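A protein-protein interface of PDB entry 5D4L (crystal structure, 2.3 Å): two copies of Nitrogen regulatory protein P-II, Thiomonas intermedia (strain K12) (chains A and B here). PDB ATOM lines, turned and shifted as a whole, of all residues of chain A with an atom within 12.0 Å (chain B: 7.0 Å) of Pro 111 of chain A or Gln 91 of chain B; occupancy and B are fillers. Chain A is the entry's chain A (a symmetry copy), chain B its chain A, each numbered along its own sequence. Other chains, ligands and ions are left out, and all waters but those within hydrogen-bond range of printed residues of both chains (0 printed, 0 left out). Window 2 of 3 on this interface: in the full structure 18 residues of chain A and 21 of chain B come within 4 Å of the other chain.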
ATOM      1  N   ALA A  11     -31.821 -19.591  -2.911  1.00  0.00           N
ATOM      2  CA  ALA A  11     -30.568 -18.861  -2.766  1.00  0.00           C
ATOM      3  C   ALA A  11     -29.564 -19.692  -1.972  1.00  0.00           C
ATOM      4  O   ALA A  11     -29.122 -19.273  -0.892  1.00  0.00           O
ATOM      5  CB  ALA A  11     -30.806 -17.521  -2.087  1.00  0.00           C
ATOM      6  N   ILE A  12     -29.215 -20.862  -2.514  1.00  0.00           N
ATOM      7  CA  ILE A  12     -28.362 -21.831  -1.826  1.00  0.00           C
ATOM      8  C   ILE A  12     -26.930 -21.813  -2.335  1.00  0.00           C
ATOM      9  O   ILE A  12     -26.681 -21.794  -3.534  1.00  0.00           O
ATOM     10  CB  ILE A  12     -28.903 -23.277  -1.973  1.00  0.00           C
ATOM     11  CG1 ILE A  12     -30.300 -23.406  -1.365  1.00  0.00           C
ATOM     12  CG2 ILE A  12     -27.963 -24.280  -1.300  1.00  0.00           C
ATOM     13  CD1 ILE A  12     -30.322 -23.341   0.129  1.00  0.00           C
ATOM     14  N   LYS A  13     -25.988 -21.830  -1.405  1.00  0.00           N
ATOM     15  CA  LYS A  13     -24.574 -21.913  -1.726  1.00  0.00           C
ATOM     16  C   LYS A  13     -24.004 -23.125  -1.000  1.00  0.00           C
ATOM     17  O   LYS A  13     -24.352 -23.393   0.154  1.00  0.00           O
ATOM     18  CB  LYS A  13     -23.852 -20.620  -1.315  1.00  0.00           C
ATOM     19  CG  LYS A  13     -22.370 -20.758  -1.063  1.00  0.00           C
ATOM     20  CD  LYS A  13     -21.771 -19.443  -0.548  1.00  0.00           C
ATOM     21  CE  LYS A  13     -20.302 -19.608  -0.138  1.00  0.00           C
ATOM     22  NZ  LYS A  13     -19.392 -19.809  -1.308  1.00  0.00           N
ATOM     23  N   LEU A  14     -23.131 -23.856  -1.672  1.00  0.00           N
ATOM     24  CA  LEU A  14     -22.597 -25.083  -1.117  1.00  0.00           C
ATOM     25  C   LEU A  14     -21.309 -24.786  -0.364  1.00  0.00           C
ATOM     26  O   LEU A  14     -20.497 -23.974  -0.801  1.00  0.00           O
ATOM     27  CB  LEU A  14     -22.370 -26.105  -2.227  1.00  0.00           C
ATOM     28  CG  LEU A  14     -23.605 -26.556  -3.016  1.00  0.00           C
ATOM     29  CD1 LEU A  14     -23.174 -27.221  -4.310  1.00  0.00           C
ATOM     30  CD2 LEU A  14     -24.502 -27.505  -2.211  1.00  0.00           C
ATOM     31  N   TYR A  15     -21.154 -25.426   0.791  1.00  0.00           N
ATOM     32  CA  TYR A  15     -19.961 -25.304   1.622  1.00  0.00           C
ATOM     33  C   TYR A  15     -19.252 -26.650   1.603  1.00  0.00           C
ATOM     34  O   TYR A  15     -19.901 -27.673   1.780  1.00  0.00           O
ATOM     35  CB  TYR A  15     -20.327 -24.912   3.066  1.00  0.00           C
ATOM     36  CG  TYR A  15     -20.748 -23.468   3.217  1.00  0.00           C
ATOM     37  CD1 TYR A  15     -21.829 -22.959   2.497  1.00  0.00           C
ATOM     38  CD2 TYR A  15     -20.063 -22.601   4.080  1.00  0.00           C
ATOM     39  CE1 TYR A  15     -22.217 -21.624   2.618  1.00  0.00           C
ATOM     40  CE2 TYR A  15     -20.446 -21.264   4.216  1.00  0.00           C
ATOM     41  CZ  TYR A  15     -21.527 -20.788   3.479  1.00  0.00           C
ATOM     42  OH  TYR A  15     -21.926 -19.481   3.591  1.00  0.00           O
ATOM     43  N   PRO A  16     -17.930 -26.666   1.373  1.00  0.00           N
ATOM     44  CA  PRO A  16     -17.254 -27.963   1.460  1.00  0.00           C
ATOM     45  C   PRO A  16     -16.905 -28.318   2.906  1.00  0.00           C
ATOM     46  O   PRO A  16     -16.501 -27.467   3.671  1.00  0.00           O
ATOM     47  CB  PRO A  16     -15.988 -27.759   0.623  1.00  0.00           C
ATOM     48  CG  PRO A  16     -15.697 -26.292   0.743  1.00  0.00           C
ATOM     49  CD  PRO A  16     -17.028 -25.587   0.919  1.00  0.00           C
ATOM     50  N   GLN A 107     -20.481 -31.780   0.492  1.00  0.00           N
ATOM     51  CA  GLN A 107     -20.894 -30.390   0.513  1.00  0.00           C
ATOM     52  C   GLN A 107     -22.219 -30.290   1.228  1.00  0.00           C
ATOM     53  O   GLN A 107     -23.003 -31.237   1.187  1.00  0.00           O
ATOM     54  CB  GLN A 107     -20.989 -29.828  -0.905  1.00  0.00           C
ATOM     55  CG  GLN A 107     -19.668 -29.986  -1.673  1.00  0.00           C
ATOM     56  CD  GLN A 107     -19.658 -29.268  -3.003  1.00  0.00           C
ATOM     57  OE1 GLN A 107     -20.709 -28.958  -3.566  1.00  0.00           O
ATOM     58  NE2 GLN A 107     -18.464 -28.990  -3.512  1.00  0.00           N
ATOM     59  N   VAL A 108     -22.458 -29.157   1.897  1.00  0.00           N
ATOM     60  CA  VAL A 108     -23.725 -28.896   2.556  1.00  0.00           C
ATOM     61  C   VAL A 108     -24.256 -27.532   2.119  1.00  0.00           C
ATOM     62  O   VAL A 108     -23.516 -26.549   2.029  1.00  0.00           O
ATOM     63  CB  VAL A 108     -23.612 -28.956   4.108  1.00  0.00           C
ATOM     64  CG1 VAL A 108     -23.224 -30.350   4.562  1.00  0.00           C
ATOM     65  CG2 VAL A 108     -22.608 -27.953   4.626  1.00  0.00           C
ATOM     66  N   GLY A 109     -25.547 -27.483   1.826  1.00  0.00           N
ATOM     67  CA  GLY A 109     -26.155 -26.283   1.281  1.00  0.00           C
ATOM     68  C   GLY A 109     -26.600 -25.342   2.382  1.00  0.00           C
ATOM     69  O   GLY A 109     -27.176 -25.773   3.375  1.00  0.00           O
ATOM     70  N   ARG A 110     -26.310 -24.056   2.209  1.00  0.00           N
ATOM     71  CA  ARG A 110     -26.738 -23.018   3.147  1.00  0.00           C
ATOM     72  C   ARG A 110     -27.367 -21.868   2.351  1.00  0.00           C
ATOM     73  O   ARG A 110     -26.868 -21.502   1.290  1.00  0.00           O
ATOM     74  CB  ARG A 110     -25.554 -22.523   4.000  1.00  0.00           C
ATOM     75  CG  ARG A 110     -25.635 -21.054   4.400  1.00  0.00           C
ATOM     76  CD  ARG A 110     -24.443 -20.593   5.246  1.00  0.00           C
ATOM     77  NE  ARG A 110     -24.709 -19.327   5.945  1.00  0.00           N
ATOM     78  CZ  ARG A 110     -24.516 -18.112   5.422  1.00  0.00           C
ATOM     79  NH1 ARG A 110     -24.047 -17.977   4.186  1.00  0.00           N
ATOM     80  NH2 ARG A 110     -24.788 -17.025   6.139  1.00  0.00           N
ATOM     81  N   PRO A 111     -28.482 -21.315   2.846  1.00  0.00           N
ATOM     82  CA  PRO A 111     -29.109 -20.176   2.163  1.00  0.00           C
ATOM     83  C   PRO A 111     -28.253 -18.918   2.263  1.00  0.00           C
ATOM     84  O   PRO A 111     -27.733 -18.629   3.340  1.00  0.00           O
ATOM     85  CB  PRO A 111     -30.434 -20.011   2.907  1.00  0.00           C
ATOM     86  CG  PRO A 111     -30.152 -20.536   4.279  1.00  0.00           C
ATOM     87  CD  PRO A 111     -29.197 -21.682   4.081  1.00  0.00           C
ATOM     88  N   ILE A 112     -28.093 -18.194   1.159  1.00  0.00           N
ATOM     89  CA  ILE A 112     -27.281 -16.974   1.160  1.00  0.00           C
ATOM     90  C   ILE A 112     -27.996 -15.831   1.892  1.00  0.00           C
ATOM     91  O   ILE A 112     -27.853 -15.664   3.111  1.00  0.00           O
ATOM     92  CB  ILE A 112     -26.927 -16.523  -0.278  1.00  0.00           C
ATOM     93  N   LEU B  35     -41.472 -35.168  -1.601  1.00  0.00           N
ATOM     94  CA  LEU B  35     -40.635 -34.139  -2.175  1.00  0.00           C
ATOM     95  C   LEU B  35     -39.717 -34.734  -3.250  1.00  0.00           C
ATOM     96  O   LEU B  35     -39.595 -34.185  -4.343  1.00  0.00           O
ATOM     97  CB  LEU B  35     -39.826 -33.451  -1.073  1.00  0.00           C
ATOM     98  CG  LEU B  35     -39.163 -32.117  -1.385  1.00  0.00           C
ATOM     99  CD1 LEU B  35     -40.086 -31.298  -2.254  1.00  0.00           C
ATOM    100  CD2 LEU B  35     -38.894 -31.390  -0.090  1.00  0.00           C
ATOM    101  N   MET B  58     -24.517 -27.387   9.400  1.00  0.00           N
ATOM    102  CA  MET B  58     -25.343 -26.311   8.854  1.00  0.00           C
ATOM    103  C   MET B  58     -24.942 -24.930   9.376  1.00  0.00           C
ATOM    104  O   MET B  58     -24.040 -24.806  10.203  1.00  0.00           O
ATOM    105  CB  MET B  58     -26.818 -26.581   9.163  1.00  0.00           C
ATOM    106  CG  MET B  58     -27.400 -27.758   8.379  1.00  0.00           C
ATOM    107  SD  MET B  58     -27.977 -27.310   6.722  1.00  0.00           S
ATOM    108  CE  MET B  58     -29.760 -27.391   6.972  1.00  0.00           C
ATOM    109  N   TYR B  59     -25.613 -23.898   8.871  1.00  0.00           N
ATOM    110  CA  TYR B  59     -25.416 -22.527   9.338  1.00  0.00           C
ATOM    111  C   TYR B  59     -25.726 -22.364  10.831  1.00  0.00           C
ATOM    112  O   TYR B  59     -26.595 -23.063  11.357  1.00  0.00           O
ATOM    113  CB  TYR B  59     -26.285 -21.577   8.518  1.00  0.00           C
ATOM    114  CG  TYR B  59     -27.738 -21.989   8.427  1.00  0.00           C
ATOM    115  CD1 TYR B  59     -28.672 -21.537   9.358  1.00  0.00           C
ATOM    116  CD2 TYR B  59     -28.185 -22.816   7.395  1.00  0.00           C
ATOM    117  CE1 TYR B  59     -30.011 -21.907   9.266  1.00  0.00           C
ATOM    118  CE2 TYR B  59     -29.512 -23.198   7.298  1.00  0.00           C
ATOM    119  CZ  TYR B  59     -30.421 -22.742   8.233  1.00  0.00           C
ATOM    120  OH  TYR B  59     -31.742 -23.111   8.131  1.00  0.00           O
ATOM    121  N   HIS B  62     -29.154 -23.128  12.937  1.00  0.00           N
ATOM    122  CA  HIS B  62     -29.994 -24.195  12.401  1.00  0.00           C
ATOM    123  C   HIS B  62     -30.343 -25.162  13.516  1.00  0.00           C
ATOM    124  O   HIS B  62     -29.496 -25.478  14.347  1.00  0.00           O
ATOM    125  CB  HIS B  62     -29.325 -24.957  11.258  1.00  0.00           C
ATOM    126  CG  HIS B  62     -30.162 -26.090  10.746  1.00  0.00           C
ATOM    127  ND1 HIS B  62     -31.442 -25.904  10.260  1.00  0.00           N
ATOM    128  CD2 HIS B  62     -29.921 -27.422  10.678  1.00  0.00           C
ATOM    129  CE1 HIS B  62     -31.950 -27.075   9.909  1.00  0.00           C
ATOM    130  NE2 HIS B  62     -31.049 -28.011  10.152  1.00  0.00           N
ATOM    131  N   LEU B  86     -33.521 -29.598  -5.372  1.00  0.00           N
ATOM    132  CA  LEU B  86     -33.885 -30.398  -4.190  1.00  0.00           C
ATOM    133  C   LEU B  86     -33.508 -29.696  -2.880  1.00  0.00           C
ATOM    134  O   LEU B  86     -34.237 -29.766  -1.890  1.00  0.00           O
ATOM    135  CB  LEU B  86     -33.231 -31.795  -4.254  1.00  0.00           C
ATOM    136  CG  LEU B  86     -33.921 -32.886  -5.097  1.00  0.00           C
ATOM    137  CD1 LEU B  86     -33.092 -34.166  -5.161  1.00  0.00           C
ATOM    138  CD2 LEU B  86     -35.343 -33.199  -4.601  1.00  0.00           C
ATOM    139  N   LEU B  87     -32.369 -29.011  -2.870  1.00  0.00           N
ATOM    140  CA  LEU B  87     -31.962 -28.288  -1.677  1.00  0.00           C
ATOM    141  C   LEU B  87     -32.894 -27.080  -1.455  1.00  0.00           C
ATOM    142  O   LEU B  87     -33.186 -26.702  -0.314  1.00  0.00           O
ATOM    143  CB  LEU B  87     -30.499 -27.854  -1.783  1.00  0.00           C
ATOM    144  CG  LEU B  87     -29.463 -28.986  -1.911  1.00  0.00           C
ATOM    145  CD1 LEU B  87     -28.048 -28.432  -1.954  1.00  0.00           C
ATOM    146  CD2 LEU B  87     -29.601 -29.994  -0.778  1.00  0.00           C
ATOM    147  N   GLU B  88     -33.368 -26.489  -2.550  1.00  0.00           N
ATOM    148  CA  GLU B  88     -34.318 -25.383  -2.475  1.00  0.00           C
ATOM    149  C   GLU B  88     -35.671 -25.870  -1.984  1.00  0.00           C
ATOM    150  O   GLU B  88     -36.355 -25.178  -1.229  1.00  0.00           O
ATOM    151  CB  GLU B  88     -34.456 -24.700  -3.830  1.00  0.00           C
ATOM    152  CG  GLU B  88     -33.238 -23.885  -4.209  1.00  0.00           C
ATOM    153  CD  GLU B  88     -33.459 -23.042  -5.447  1.00  0.00           C
ATOM    154  OE1 GLU B  88     -34.599 -23.044  -5.965  1.00  0.00           O
ATOM    155  OE2 GLU B  88     -32.496 -22.372  -5.887  1.00  0.00           O
ATOM    156  N   GLY B  89     -36.046 -27.073  -2.400  1.00  0.00           N
ATOM    157  CA  GLY B  89     -37.241 -27.715  -1.893  1.00  0.00           C
ATOM    158  C   GLY B  89     -37.202 -27.985  -0.402  1.00  0.00           C
ATOM    159  O   GLY B  89     -38.197 -27.775   0.286  1.00  0.00           O
ATOM    160  N   PHE B  90     -36.066 -28.448   0.115  1.00  0.00           N
ATOM    161  CA  PHE B  90     -36.000 -28.804   1.529  1.00  0.00           C
ATOM    162  C   PHE B  90     -35.828 -27.601   2.452  1.00  0.00           C
ATOM    163  O   PHE B  90     -36.134 -27.690   3.629  1.00  0.00           O
ATOM    164  CB  PHE B  90     -34.860 -29.791   1.785  1.00  0.00           C
ATOM    165  CG  PHE B  90     -35.226 -31.218   1.507  1.00  0.00           C
ATOM    166  CD1 PHE B  90     -35.922 -31.963   2.450  1.00  0.00           C
ATOM    167  CD2 PHE B  90     -34.872 -31.816   0.306  1.00  0.00           C
ATOM    168  CE1 PHE B  90     -36.262 -33.289   2.199  1.00  0.00           C
ATOM    169  CE2 PHE B  90     -35.210 -33.138   0.045  1.00  0.00           C
ATOM    170  CZ  PHE B  90     -35.913 -33.874   0.989  1.00  0.00           C
ATOM    171  N   GLN B  91     -35.351 -26.480   1.926  1.00  0.00           N
ATOM    172  CA  GLN B  91     -34.984 -25.348   2.788  1.00  0.00           C
ATOM    173  C   GLN B  91     -36.125 -24.764   3.655  1.00  0.00           C
ATOM    174  O   GLN B  91     -35.902 -24.465   4.830  1.00  0.00           O
ATOM    175  CB  GLN B  91     -34.360 -24.211   1.964  1.00  0.00           C
ATOM    176  CG  GLN B  91     -33.829 -23.103   2.862  1.00  0.00           C
ATOM    177  CD  GLN B  91     -32.732 -23.579   3.831  1.00  0.00           C
ATOM    178  OE1 GLN B  91     -32.150 -24.662   3.675  1.00  0.00           O
ATOM    179  NE2 GLN B  91     -32.498 -22.791   4.876  1.00  0.00           N
ATOM    180  N   PRO B  92     -37.337 -24.598   3.093  1.00  0.00           N
ATOM    181  CA  PRO B  92     -38.411 -24.160   3.994  1.00  0.00           C
ATOM    182  C   PRO B  92     -38.594 -25.120   5.152  1.00  0.00           C
ATOM    183  O   PRO B  92     -38.861 -24.692   6.286  1.00  0.00           O
ATOM    184  CB  PRO B  92     -39.649 -24.154   3.089  1.00  0.00           C
ATOM    185  CG  PRO B  92     -39.108 -23.880   1.735  1.00  0.00           C
ATOM    186  CD  PRO B  92     -37.781 -24.615   1.685  1.00  0.00           C
ATOM    187  N   PHE B  93     -38.434 -26.410   4.864  1.00  0.00           N
ATOM    188  CA  PHE B  93     -38.586 -27.443   5.878  1.00  0.00           C
ATOM    189  C   PHE B  93     -37.518 -27.318   6.968  1.00  0.00           C
ATOM    190  O   PHE B  93     -37.816 -27.479   8.161  1.00  0.00           O
ATOM    191  CB  PHE B  93     -38.534 -28.846   5.255  1.00  0.00           C
ATOM    192  CG  PHE B  93     -38.525 -29.942   6.271  1.00  0.00           C
ATOM    193  CD1 PHE B  93     -39.706 -30.359   6.859  1.00  0.00           C
ATOM    194  CD2 PHE B  93     -37.328 -30.525   6.678  1.00  0.00           C
ATOM    195  CE1 PHE B  93     -39.700 -31.350   7.825  1.00  0.00           C
ATOM    196  CE2 PHE B  93     -37.313 -31.517   7.646  1.00  0.00           C
ATOM    197  CZ  PHE B  93     -38.497 -31.929   8.217  1.00  0.00           C
ATOM    198  N   PHE B  94     -36.279 -27.050   6.562  1.00  0.00           N
ATOM    199  CA  PHE B  94     -35.173 -27.001   7.520  1.00  0.00           C
ATOM    200  C   PHE B  94     -35.206 -25.738   8.366  1.00  0.00           C
ATOM    201  O   PHE B  94     -34.600 -25.684   9.435  1.00  0.00           O
ATOM    202  CB  PHE B  94     -33.829 -27.126   6.799  1.00  0.00           C
ATOM    203  CG  PHE B  94     -33.553 -28.520   6.316  1.00  0.00           C
ATOM    204  CD1 PHE B  94     -33.906 -29.612   7.101  1.00  0.00           C
ATOM    205  CD2 PHE B  94     -32.988 -28.750   5.070  1.00  0.00           C
ATOM    206  CE1 PHE B  94     -33.693 -30.899   6.662  1.00  0.00           C
ATOM    207  CE2 PHE B  94     -32.763 -30.047   4.631  1.00  0.00           C
ATOM    208  CZ  PHE B  94     -33.116 -31.118   5.427  1.00  0.00           C
ATOM    209  N   GLU B  95     -35.941 -24.733   7.905  1.00  0.00           N
ATOM    210  CA  GLU B  95     -36.103 -23.509   8.686  1.00  0.00           C
ATOM    211  C   GLU B  95     -36.889 -23.745   9.972  1.00  0.00           C
ATOM    212  O   GLU B  95     -36.752 -22.992  10.928  1.00  0.00           O
ATOM    213  CB  GLU B  95     -36.778 -22.431   7.836  1.00  0.00           C
ATOM    214  CG  GLU B  95     -35.780 -21.715   6.946  1.00  0.00           C
ATOM    215  CD  GLU B  95     -36.420 -20.912   5.829  1.00  0.00           C
ATOM    216  OE1 GLU B  95     -35.674 -20.554   4.891  1.00  0.00           O
ATOM    217  OE2 GLU B  95     -37.647 -20.638   5.880  1.00  0.00           O
ATOM    218  N   ALA B  96     -37.692 -24.806  10.007  1.00  0.00           N
ATOM    219  CA  ALA B  96     -38.502 -25.095  11.188  1.00  0.00           C
ATOM    220  C   ALA B  96     -38.254 -26.501  11.756  1.00  0.00           C
ATOM    221  O   ALA B  96     -38.867 -26.897  12.752  1.00  0.00           O
ATOM    222  CB  ALA B  96     -39.980 -24.914  10.858  1.00  0.00           C
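Among the printed residues, merely in contact across the chains: Leu 14 of chain A with Leu 87 of chain B, Arg 110 of chain A with Tyr 59 of chain B, Pro 111 of chain A with Tyr 59 of chain B and Pro 111 of chain A with Gln 91 of chain B.
Pro 111 of chain A touches just these residues of chain B: Tyr 59 and Gln 91.
Tyr 59 of chain B touches two residues of chain A.
Of chain A, only Leu 14 (3.7 Å) comes within 4 Å of Leu 87 of chain B.
No residue of chain A comes within 4 Å of Gly 89 of chain B.
Of the printed residues of chain A, Met 58 of chain B touches Gly 109.
Printed residues of chain B within 4 Å of Arg 110 of chain A: Tyr 59 (3.8 Å).
Printed residues of chain B within 4 Å of Leu 14 of chain A: Leu 87.
Printed residues of chain B within 4 Å of Gly 109 of chain A: Met 58.
The nearest residue of chain B that does not touch Pro 111 of chain A is Glu 95 of chain B (5.6 Å).
The nearest printed residue of chain B that does not touch Arg 110 of chain A is Gln 91 of chain B (5.7 Å).
Of the 15 printed residues of chain B, 4 touch a printed residue of chain A.
Along chain B the printed residues that touch a printed residue of chain A span positions 58 to 91.
Printed residues of chain A that touch a printed residue of chain B: Leu 14, Gly 109, Arg 110 and Pro 111.
Among the printed residues, no Asp or Glu carboxylate lies within 4 Å of a Lys or Arg side-chain nitrogen of the other chain.
O of Gly 109 of chain A lies close to SD of Met 58 of chain B, 3.8 Å away.
The side-chain amide nitrogen of Gln 91 of chain B lies within hydrogen-bond range of the side-chain hydroxyl of Tyr 59 of chain B.
The backbone NH (N) of Lys 13 of chain A sits at hydrogen-bond distance from the backbone carbonyl oxygen (O) of Arg 110 of chain A (2.9 Å).
The guanidinium group (NH1) of Arg 110 of chain A sits at hydrogen-bond distance from the side-chain hydroxyl (OH) of Tyr 15 of chain A (2.7 Å).
No position is printed for both chains.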
